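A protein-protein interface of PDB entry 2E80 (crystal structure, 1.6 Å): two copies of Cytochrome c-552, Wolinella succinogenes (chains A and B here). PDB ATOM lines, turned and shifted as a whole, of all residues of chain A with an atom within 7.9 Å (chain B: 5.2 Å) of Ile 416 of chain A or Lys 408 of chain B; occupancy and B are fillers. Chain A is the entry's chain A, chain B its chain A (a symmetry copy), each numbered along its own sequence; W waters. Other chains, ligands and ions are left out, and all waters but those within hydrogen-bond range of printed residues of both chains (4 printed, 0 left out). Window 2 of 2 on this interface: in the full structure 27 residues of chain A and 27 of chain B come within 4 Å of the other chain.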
ATOM      1  N   GLU A 343      21.292   5.590  18.968  1.00  0.00           N
ATOM      2  CA  GLU A 343      20.745   4.398  18.328  1.00  0.00           C
ATOM      3  C   GLU A 343      20.368   3.358  19.383  1.00  0.00           C
ATOM      4  O   GLU A 343      19.397   2.618  19.219  1.00  0.00           O
ATOM      5  CB  GLU A 343      21.767   3.845  17.329  1.00  0.00           C
ATOM      6  CG  GLU A 343      21.941   4.780  16.136  1.00  0.00           C
ATOM      7  CD  GLU A 343      23.221   4.554  15.347  1.00  0.00           C
ATOM      8  OE1 GLU A 343      24.053   3.715  15.751  1.00  0.00           O
ATOM      9  OE2 GLU A 343      23.393   5.236  14.315  1.00  0.00           O
ATOM     10  N   LEU A 350      12.017   0.850  21.241  1.00  0.00           N
ATOM     11  CA  LEU A 350      11.327  -0.146  20.434  1.00  0.00           C
ATOM     12  C   LEU A 350      11.105  -1.464  21.169  1.00  0.00           C
ATOM     13  O   LEU A 350      10.359  -2.324  20.698  1.00  0.00           O
ATOM     14  CB  LEU A 350      12.103  -0.389  19.140  1.00  0.00           C
ATOM     15  CG  LEU A 350      12.257   0.845  18.243  1.00  0.00           C
ATOM     16  CD1 LEU A 350      13.178   0.521  17.083  1.00  0.00           C
ATOM     17  CD2 LEU A 350      10.887   1.292  17.744  1.00  0.00           C
ATOM     18  N   ARG A 403      27.954   0.210  16.570  1.00  0.00           N
ATOM     19  CA  ARG A 403      26.980   0.647  15.576  1.00  0.00           C
ATOM     20  C   ARG A 403      26.603  -0.419  14.552  1.00  0.00           C
ATOM     21  O   ARG A 403      25.461  -0.459  14.097  1.00  0.00           O
ATOM     22  CB  ARG A 403      27.471   1.918  14.880  1.00  0.00           C
ATOM     23  CG  ARG A 403      27.649   3.073  15.858  1.00  0.00           C
ATOM     24  CD  ARG A 403      27.816   4.390  15.139  1.00  0.00           C
ATOM     25  NE  ARG A 403      26.626   4.713  14.363  1.00  0.00           N
ATOM     26  CZ  ARG A 403      26.636   4.992  13.065  1.00  0.00           C
ATOM     27  NH1 ARG A 403      27.780   4.985  12.393  1.00  0.00           N
ATOM     28  NH2 ARG A 403      25.503   5.273  12.439  1.00  0.00           N
ATOM     29  N   LEU A 406      24.218  -2.492  16.283  1.00  0.00           N
ATOM     30  CA  LEU A 406      22.983  -1.739  16.481  1.00  0.00           C
ATOM     31  C   LEU A 406      22.091  -1.743  15.245  1.00  0.00           C
ATOM     32  O   LEU A 406      20.865  -1.735  15.362  1.00  0.00           O
ATOM     33  CB  LEU A 406      23.304  -0.299  16.883  1.00  0.00           C
ATOM     34  CG  LEU A 406      23.619  -0.118  18.370  1.00  0.00           C
ATOM     35  CD1 LEU A 406      24.316   1.214  18.592  1.00  0.00           C
ATOM     36  CD2 LEU A 406      22.329  -0.204  19.182  1.00  0.00           C
ATOM     37  N   VAL A 407      22.691  -1.750  14.060  1.00  0.00           N
ATOM     38  CA  VAL A 407      21.887  -1.763  12.843  1.00  0.00           C
ATOM     39  C   VAL A 407      21.015  -3.012  12.855  1.00  0.00           C
ATOM     40  O   VAL A 407      19.843  -2.972  12.481  1.00  0.00           O
ATOM     41  CB  VAL A 407      22.755  -1.801  11.570  1.00  0.00           C
ATOM     42  CG1 VAL A 407      21.855  -1.865  10.338  1.00  0.00           C
ATOM     43  CG2 VAL A 407      23.660  -0.585  11.507  1.00  0.00           C
ATOM     44  N   LYS A 408      21.592  -4.121  13.303  1.00  0.00           N
ATOM     45  CA  LYS A 408      20.867  -5.381  13.350  1.00  0.00           C
ATOM     46  C   LYS A 408      19.779  -5.398  14.416  1.00  0.00           C
ATOM     47  O   LYS A 408      18.703  -5.956  14.197  1.00  0.00           O
ATOM     48  CB  LYS A 408      21.853  -6.529  13.555  1.00  0.00           C
ATOM     49  CG  LYS A 408      22.861  -6.613  12.421  1.00  0.00           C
ATOM     50  CD  LYS A 408      23.888  -7.695  12.634  1.00  0.00           C
ATOM     51  CE  LYS A 408      24.897  -7.686  11.500  1.00  0.00           C
ATOM     52  NZ  LYS A 408      25.957  -8.706  11.700  1.00  0.00           N
ATOM     53  N   VAL A 409      20.045  -4.788  15.568  1.00  0.00           N
ATOM     54  CA  VAL A 409      19.039  -4.745  16.623  1.00  0.00           C
ATOM     55  C   VAL A 409      17.889  -3.861  16.151  1.00  0.00           C
ATOM     56  O   VAL A 409      16.716  -4.202  16.326  1.00  0.00           O
ATOM     57  CB  VAL A 409      19.614  -4.186  17.945  1.00  0.00           C
ATOM     58  CG1 VAL A 409      18.498  -4.031  18.973  1.00  0.00           C
ATOM     59  CG2 VAL A 409      20.683  -5.126  18.482  1.00  0.00           C
ATOM     60  N   LEU A 410      18.226  -2.727  15.548  1.00  0.00           N
ATOM     61  CA  LEU A 410      17.210  -1.812  15.036  1.00  0.00           C
ATOM     62  C   LEU A 410      16.371  -2.509  13.966  1.00  0.00           C
ATOM     63  O   LEU A 410      15.146  -2.378  13.932  1.00  0.00           O
ATOM     64  CB  LEU A 410      17.879  -0.562  14.454  1.00  0.00           C
ATOM     65  CG  LEU A 410      18.486   0.367  15.506  1.00  0.00           C
ATOM     66  CD1 LEU A 410      19.265   1.486  14.824  1.00  0.00           C
ATOM     67  CD2 LEU A 410      17.369   0.936  16.379  1.00  0.00           C
ATOM     68  N   ALA A 411      17.035  -3.264  13.099  1.00  0.00           N
ATOM     69  CA  ALA A 411      16.337  -3.979  12.038  1.00  0.00           C
ATOM     70  C   ALA A 411      15.333  -4.973  12.614  1.00  0.00           C
ATOM     71  O   ALA A 411      14.212  -5.090  12.117  1.00  0.00           O
ATOM     72  CB  ALA A 411      17.343  -4.705  11.145  1.00  0.00           C
ATOM     73  N   LYS A 412      15.733  -5.689  13.661  1.00  0.00           N
ATOM     74  CA  LYS A 412      14.836  -6.666  14.269  1.00  0.00           C
ATOM     75  C   LYS A 412      13.544  -6.003  14.721  1.00  0.00           C
ATOM     76  O   LYS A 412      12.466  -6.596  14.631  1.00  0.00           O
ATOM     77  CB  LYS A 412      15.488  -7.344  15.477  1.00  0.00           C
ATOM     78  CG  LYS A 412      14.501  -8.226  16.233  1.00  0.00           C
ATOM     79  CD  LYS A 412      15.061  -8.799  17.518  1.00  0.00           C
ATOM     80  CE  LYS A 412      13.951  -9.513  18.281  1.00  0.00           C
ATOM     81  NZ  LYS A 412      14.425 -10.153  19.532  1.00  0.00           N
ATOM     82  N   TYR A 413      13.658  -4.769  15.201  1.00  0.00           N
ATOM     83  CA  TYR A 413      12.497  -4.029  15.676  1.00  0.00           C
ATOM     84  C   TYR A 413      11.870  -3.111  14.632  1.00  0.00           C
ATOM     85  O   TYR A 413      11.110  -2.200  14.968  1.00  0.00           O
ATOM     86  CB  TYR A 413      12.871  -3.261  16.946  1.00  0.00           C
ATOM     87  CG  TYR A 413      13.088  -4.195  18.113  1.00  0.00           C
ATOM     88  CD1 TYR A 413      12.003  -4.742  18.794  1.00  0.00           C
ATOM     89  CD2 TYR A 413      14.371  -4.603  18.481  1.00  0.00           C
ATOM     90  CE1 TYR A 413      12.185  -5.674  19.810  1.00  0.00           C
ATOM     91  CE2 TYR A 413      14.567  -5.541  19.498  1.00  0.00           C
ATOM     92  CZ  TYR A 413      13.467  -6.074  20.154  1.00  0.00           C
ATOM     93  OH  TYR A 413      13.638  -7.023  21.134  1.00  0.00           O
ATOM     94  N   GLY A 414      12.198  -3.364  13.368  1.00  0.00           N
ATOM     95  CA  GLY A 414      11.639  -2.606  12.259  1.00  0.00           C
ATOM     96  C   GLY A 414      12.098  -1.182  12.020  1.00  0.00           C
ATOM     97  O   GLY A 414      11.394  -0.409  11.367  1.00  0.00           O
ATOM     98  N   ALA A 415      13.277  -0.826  12.513  1.00  0.00           N
ATOM     99  CA  ALA A 415      13.768   0.535  12.333  1.00  0.00           C
ATOM    100  C   ALA A 415      15.171   0.574  11.740  1.00  0.00           C
ATOM    101  O   ALA A 415      15.998   1.382  12.150  1.00  0.00           O
ATOM    102  CB  ALA A 415      13.751   1.264  13.666  1.00  0.00           C
ATOM    103  N   ILE A 416      15.435  -0.284  10.762  1.00  0.00           N
ATOM    104  CA  ILE A 416      16.761  -0.324  10.158  1.00  0.00           C
ATOM    105  C   ILE A 416      17.181   1.003   9.521  1.00  0.00           C
ATOM    106  O   ILE A 416      18.373   1.297   9.432  1.00  0.00           O
ATOM    107  CB  ILE A 416      16.859  -1.438   9.097  1.00  0.00           C
ATOM    108  CG1 ILE A 416      18.332  -1.739   8.807  1.00  0.00           C
ATOM    109  CG2 ILE A 416      16.152  -1.005   7.815  1.00  0.00           C
ATOM    110  CD1 ILE A 416      18.549  -2.973   7.959  1.00  0.00           C
ATOM    111  N   ASP A 417      16.210   1.804   9.092  1.00  0.00           N
ATOM    112  CA  ASP A 417      16.521   3.085   8.455  1.00  0.00           C
ATOM    113  C   ASP A 417      16.527   4.271   9.411  1.00  0.00           C
ATOM    114  O   ASP A 417      16.501   5.425   8.979  1.00  0.00           O
ATOM    115  CB  ASP A 417      15.545   3.360   7.309  1.00  0.00           C
ATOM    116  CG  ASP A 417      15.637   2.318   6.211  1.00  0.00           C
ATOM    117  OD1 ASP A 417      16.766   2.026   5.768  1.00  0.00           O
ATOM    118  OD2 ASP A 417      14.584   1.792   5.792  1.00  0.00           O
ATOM    119  N   TYR A 418      16.558   3.990  10.707  1.00  0.00           N
ATOM    120  CA  TYR A 418      16.585   5.049  11.705  1.00  0.00           C
ATOM    121  C   TYR A 418      17.848   5.889  11.539  1.00  0.00           C
ATOM    122  O   TYR A 418      18.935   5.354  11.316  1.00  0.00           O
ATOM    123  CB  TYR A 418      16.553   4.441  13.112  1.00  0.00           C
ATOM    124  CG  TYR A 418      16.833   5.423  14.231  1.00  0.00           C
ATOM    125  CD1 TYR A 418      15.879   6.361  14.626  1.00  0.00           C
ATOM    126  CD2 TYR A 418      18.052   5.407  14.902  1.00  0.00           C
ATOM    127  CE1 TYR A 418      16.137   7.255  15.664  1.00  0.00           C
ATOM    128  CE2 TYR A 418      18.320   6.292  15.937  1.00  0.00           C
ATOM    129  CZ  TYR A 418      17.362   7.212  16.314  1.00  0.00           C
ATOM    130  OH  TYR A 418      17.635   8.080  17.345  1.00  0.00           O
ATOM    131  N   VAL A 419      17.695   7.207  11.641  1.00  0.00           N
ATOM    132  CA  VAL A 419      18.819   8.129  11.528  1.00  0.00           C
ATOM    133  C   VAL A 419      18.936   8.879  12.848  1.00  0.00           C
ATOM    134  O   VAL A 419      18.047   9.649  13.210  1.00  0.00           O
ATOM    135  CB  VAL A 419      18.604   9.162  10.395  1.00  0.00           C
ATOM    136  CG1 VAL A 419      19.800  10.106  10.322  1.00  0.00           C
ATOM    137  CG2 VAL A 419      18.408   8.450   9.069  1.00  0.00           C
ATOM    138  N   ALA A 420      20.029   8.644  13.570  1.00  0.00           N
ATOM    139  CA  ALA A 420      20.250   9.305  14.849  1.00  0.00           C
ATOM    140  C   ALA A 420      20.179  10.818  14.659  1.00  0.00           C
ATOM    141  O   ALA A 420      20.744  11.364  13.708  1.00  0.00           O
ATOM    142  CB  ALA A 420      21.610   8.907  15.412  1.00  0.00           C
ATOM    143  N   ILE B 404      28.568  -0.200   7.632  1.00  0.00           N
ATOM    144  CA  ILE B 404      27.276   0.155   8.214  1.00  0.00           C
ATOM    145  C   ILE B 404      26.240   0.152   7.091  1.00  0.00           C
ATOM    146  O   ILE B 404      25.134  -0.374   7.250  1.00  0.00           O
ATOM    147  CB  ILE B 404      27.320   1.557   8.865  1.00  0.00           C
ATOM    148  CG1 ILE B 404      28.202   1.521  10.118  1.00  0.00           C
ATOM    149  CG2 ILE B 404      25.907   2.028   9.207  1.00  0.00           C
ATOM    150  CD1 ILE B 404      27.639   0.684  11.253  1.00  0.00           C
ATOM    151  N   LYS B 405      26.601   0.729   5.949  1.00  0.00           N
ATOM    152  CA  LYS B 405      25.684   0.767   4.814  1.00  0.00           C
ATOM    153  C   LYS B 405      25.465  -0.634   4.250  1.00  0.00           C
ATOM    154  O   LYS B 405      24.370  -0.967   3.797  1.00  0.00           O
ATOM    155  CB  LYS B 405      26.224   1.707   3.731  1.00  0.00           C
ATOM    156  CG  LYS B 405      26.213   3.163   4.178  1.00  0.00           C
ATOM    157  CD  LYS B 405      26.763   4.112   3.129  1.00  0.00           C
ATOM    158  CE  LYS B 405      26.638   5.549   3.614  1.00  0.00           C
ATOM    159  NZ  LYS B 405      27.260   6.534   2.691  1.00  0.00           N
ATOM    160  N   LEU B 406      26.505  -1.460   4.294  1.00  0.00           N
ATOM    161  CA  LEU B 406      26.403  -2.826   3.788  1.00  0.00           C
ATOM    162  C   LEU B 406      25.429  -3.677   4.594  1.00  0.00           C
ATOM    163  O   LEU B 406      24.762  -4.552   4.042  1.00  0.00           O
ATOM    164  CB  LEU B 406      27.782  -3.487   3.777  1.00  0.00           C
ATOM    165  CG  LEU B 406      28.639  -3.130   2.560  1.00  0.00           C
ATOM    166  CD1 LEU B 406      30.093  -3.475   2.833  1.00  0.00           C
ATOM    167  CD2 LEU B 406      28.120  -3.873   1.332  1.00  0.00           C
ATOM    168  N   VAL B 407      25.343  -3.435   5.898  1.00  0.00           N
ATOM    169  CA  VAL B 407      24.420  -4.213   6.717  1.00  0.00           C
ATOM    170  C   VAL B 407      23.009  -4.010   6.180  1.00  0.00           C
ATOM    171  O   VAL B 407      22.218  -4.950   6.102  1.00  0.00           O
ATOM    172  CB  VAL B 407      24.435  -3.770   8.194  1.00  0.00           C
ATOM    173  CG1 VAL B 407      23.415  -4.587   8.984  1.00  0.00           C
ATOM    174  CG2 VAL B 407      25.822  -3.936   8.785  1.00  0.00           C
ATOM    175  N   LYS B 408      22.704  -2.777   5.794  1.00  0.00           N
ATOM    176  CA  LYS B 408      21.383  -2.454   5.276  1.00  0.00           C
ATOM    177  C   LYS B 408      21.126  -3.054   3.901  1.00  0.00           C
ATOM    178  O   LYS B 408      20.013  -3.500   3.616  1.00  0.00           O
ATOM    179  CB  LYS B 408      21.201  -0.938   5.256  1.00  0.00           C
ATOM    180  CG  LYS B 408      21.314  -0.340   6.649  1.00  0.00           C
ATOM    181  CD  LYS B 408      21.206   1.163   6.647  1.00  0.00           C
ATOM    182  CE  LYS B 408      21.387   1.700   8.055  1.00  0.00           C
ATOM    183  NZ  LYS B 408      21.338   3.183   8.088  1.00  0.00           N
ATOM    184  N   VAL B 409      22.143  -3.076   3.044  1.00  0.00           N
ATOM    185  CA  VAL B 409      21.972  -3.658   1.719  1.00  0.00           C
ATOM    186  C   VAL B 409      21.771  -5.162   1.879  1.00  0.00           C
ATOM    187  O   VAL B 409      20.903  -5.757   1.234  1.00  0.00           O
ATOM    188  CB  VAL B 409      23.195  -3.393   0.810  1.00  0.00           C
ATOM    189  CG1 VAL B 409      23.031  -4.135  -0.513  1.00  0.00           C
ATOM    190  CG2 VAL B 409      23.332  -1.901   0.551  1.00  0.00           C
ATOM    191  N   LEU B 410      22.571  -5.775   2.744  1.00  0.00           N
ATOM    192  CA  LEU B 410      22.456  -7.208   2.995  1.00  0.00           C
ATOM    193  C   LEU B 410      21.070  -7.531   3.554  1.00  0.00           C
ATOM    194  O   LEU B 410      20.438  -8.513   3.160  1.00  0.00           O
ATOM    195  CB  LEU B 410      23.541  -7.654   3.981  1.00  0.00           C
ATOM    196  CG  LEU B 410      24.953  -7.657   3.394  1.00  0.00           C
ATOM    197  CD1 LEU B 410      25.971  -7.952   4.489  1.00  0.00           C
ATOM    198  CD2 LEU B 410      25.032  -8.702   2.283  1.00  0.00           C
ATOM    199  N   ALA B 411      20.593  -6.690   4.464  1.00  0.00           N
ATOM    200  CA  ALA B 411      19.281  -6.897   5.062  1.00  0.00           C
ATOM    201  C   ALA B 411      18.183  -6.866   4.002  1.00  0.00           C
ATOM    202  O   ALA B 411      17.264  -7.686   4.029  1.00  0.00           O
ATOM    203  CB  ALA B 411      19.015  -5.832   6.125  1.00  0.00           C
ATOM    204  N   LYS B 412      18.278  -5.924   3.069  1.00  0.00           N
ATOM    205  CA  LYS B 412      17.267  -5.821   2.022  1.00  0.00           C
ATOM    206  C   LYS B 412      17.160  -7.126   1.248  1.00  0.00           C
ATOM    207  O   LYS B 412      16.068  -7.527   0.838  1.00  0.00           O
ATOM    208  CB  LYS B 412      17.596  -4.694   1.040  1.00  0.00           C
ATOM    209  CG  LYS B 412      16.656  -4.695  -0.160  1.00  0.00           C
ATOM    210  CD  LYS B 412      17.035  -3.691  -1.229  1.00  0.00           C
ATOM    211  CE  LYS B 412      16.147  -3.894  -2.452  1.00  0.00           C
ATOM    212  NZ  LYS B 412      16.415  -2.913  -3.532  1.00  0.00           N
ATOM    213  N   ILE B 416      20.971 -10.231   6.519  1.00  0.00           N
ATOM    214  CA  ILE B 416      21.496  -9.342   7.549  1.00  0.00           C
ATOM    215  C   ILE B 416      22.471 -10.029   8.507  1.00  0.00           C
ATOM    216  O   ILE B 416      23.348  -9.375   9.073  1.00  0.00           O
ATOM    217  CB  ILE B 416      20.358  -8.705   8.371  1.00  0.00           C
ATOM    218  CG1 ILE B 416      20.893  -7.483   9.123  1.00  0.00           C
ATOM    219  CG2 ILE B 416      19.792  -9.721   9.360  1.00  0.00           C
ATOM    220  CD1 ILE B 416      19.815  -6.644   9.773  1.00  0.00           C
HETATM  221  O   HOH W   1      20.041   5.324   8.820  1.00  0.00           O
HETATM  222  O   HOH W   2      18.950   3.561   6.045  1.00  0.00           O
HETATM  223  O   HOH W   3      26.089  -8.992   8.514  1.00  0.00           O
HETATM  224  O   HOH W   4      20.046   2.937  11.007  1.00  0.00           O
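Water W1 lies within hydrogen-bond range of NZ of Lys 408 of chain B (2.6 Å) and O of Tyr 418 of chain A (2.7 Å). Water W4 lies within hydrogen-bond range of O of Tyr 418 of chain A (2.7 Å), O of Ile 416 of chain A (2.8 Å) and NZ of Lys 408 of chain B (3.2 Å). Water W2 lies within hydrogen-bond range of the side-chain carboxylate (OD1) of Asp 417 of chain A (2.7 Å) and the side-chain amino group (NZ) of Lys 408 of chain B (3.2 Å). Water W3 lies within hydrogen-bond range of O of Ile 416 of chain B (2.8 Å) and NZ of Lys 408 of chain A (3.2 Å).
Hydrophobic or aromatic side chains of chain A that line the printed part of chain B: Val 407, Ala 411 and Ile 416. Of the 10 printed residues of chain B, 5 touch a printed residue of chain A. Printed residues of chain B that touch a printed residue of chain A: Ile 404, Val 407, Lys 408, Ala 411 and Ile 416. Hydrophobic or aromatic side chains of chain B within 4 Å of the printed part of chain A: Ile 404, Val 407, Ala 411 and Ile 416. Among the printed residues, 6 pairs touch across the chains. Among the printed residues, no Asp or Glu carboxylate lies within 4 Å of a Lys or Arg side-chain nitrogen of the other chain.
The side-chain carboxylate (OE2) of Glu 343 of chain A is in salt-bridge range of the guanidinium group (NH2) of Arg 403 of chain A (2.8 Å).
Of the printed residues of chain B, Lys 408 of chain A touches Ile 416. Printed residues of chain B within 4 Å of Ala 411 of chain A: Ile 416 (3.4 Å). Ile 416 of chain A touches two residues of chain B. Of chain A, only Ile 416 (3.3 Å) comes within 4 Å of Lys 408 of chain B. Of the printed residues of chain A, Ala 411 of chain B touches Ile 416 (3.4 Å). The nearest residue of chain B that does not touch Ile 416 of chain A is Ile 416 of chain B (4.3 Å). The nearest residue of chain A that does not touch Lys 408 of chain B is Val 407 of chain A (4.03 Å). The nearest printed residue of chain B that does not touch Lys 408 of chain A is Val 407 of chain B (4.03 Å).
Val 407 of chain A touches its own counterpart, Val 407 of chain B. Lys 408 of chain A touches Ile 416 of chain B, and with the chains exchanged Ile 416 of chain A touches Lys 408 of chain B. Ala 411 of chain A touches Ile 416 of chain B, and with the chains exchanged Ile 416 of chain A touches Ala 411 of chain B.
Among the printed residues, merely in contact across the chains: Arg 403 of chain A with Ile 404 of chain B, Val 407 of chain A with Val 407 of chain B, Lys 408 of chain A with Ile 416 of chain B, Ala 411 of chain A with Ile 416 of chain B, Ile 416 of chain A with Lys 408 of chain B and Ile 416 of chain A with Ala 411 of chain B.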
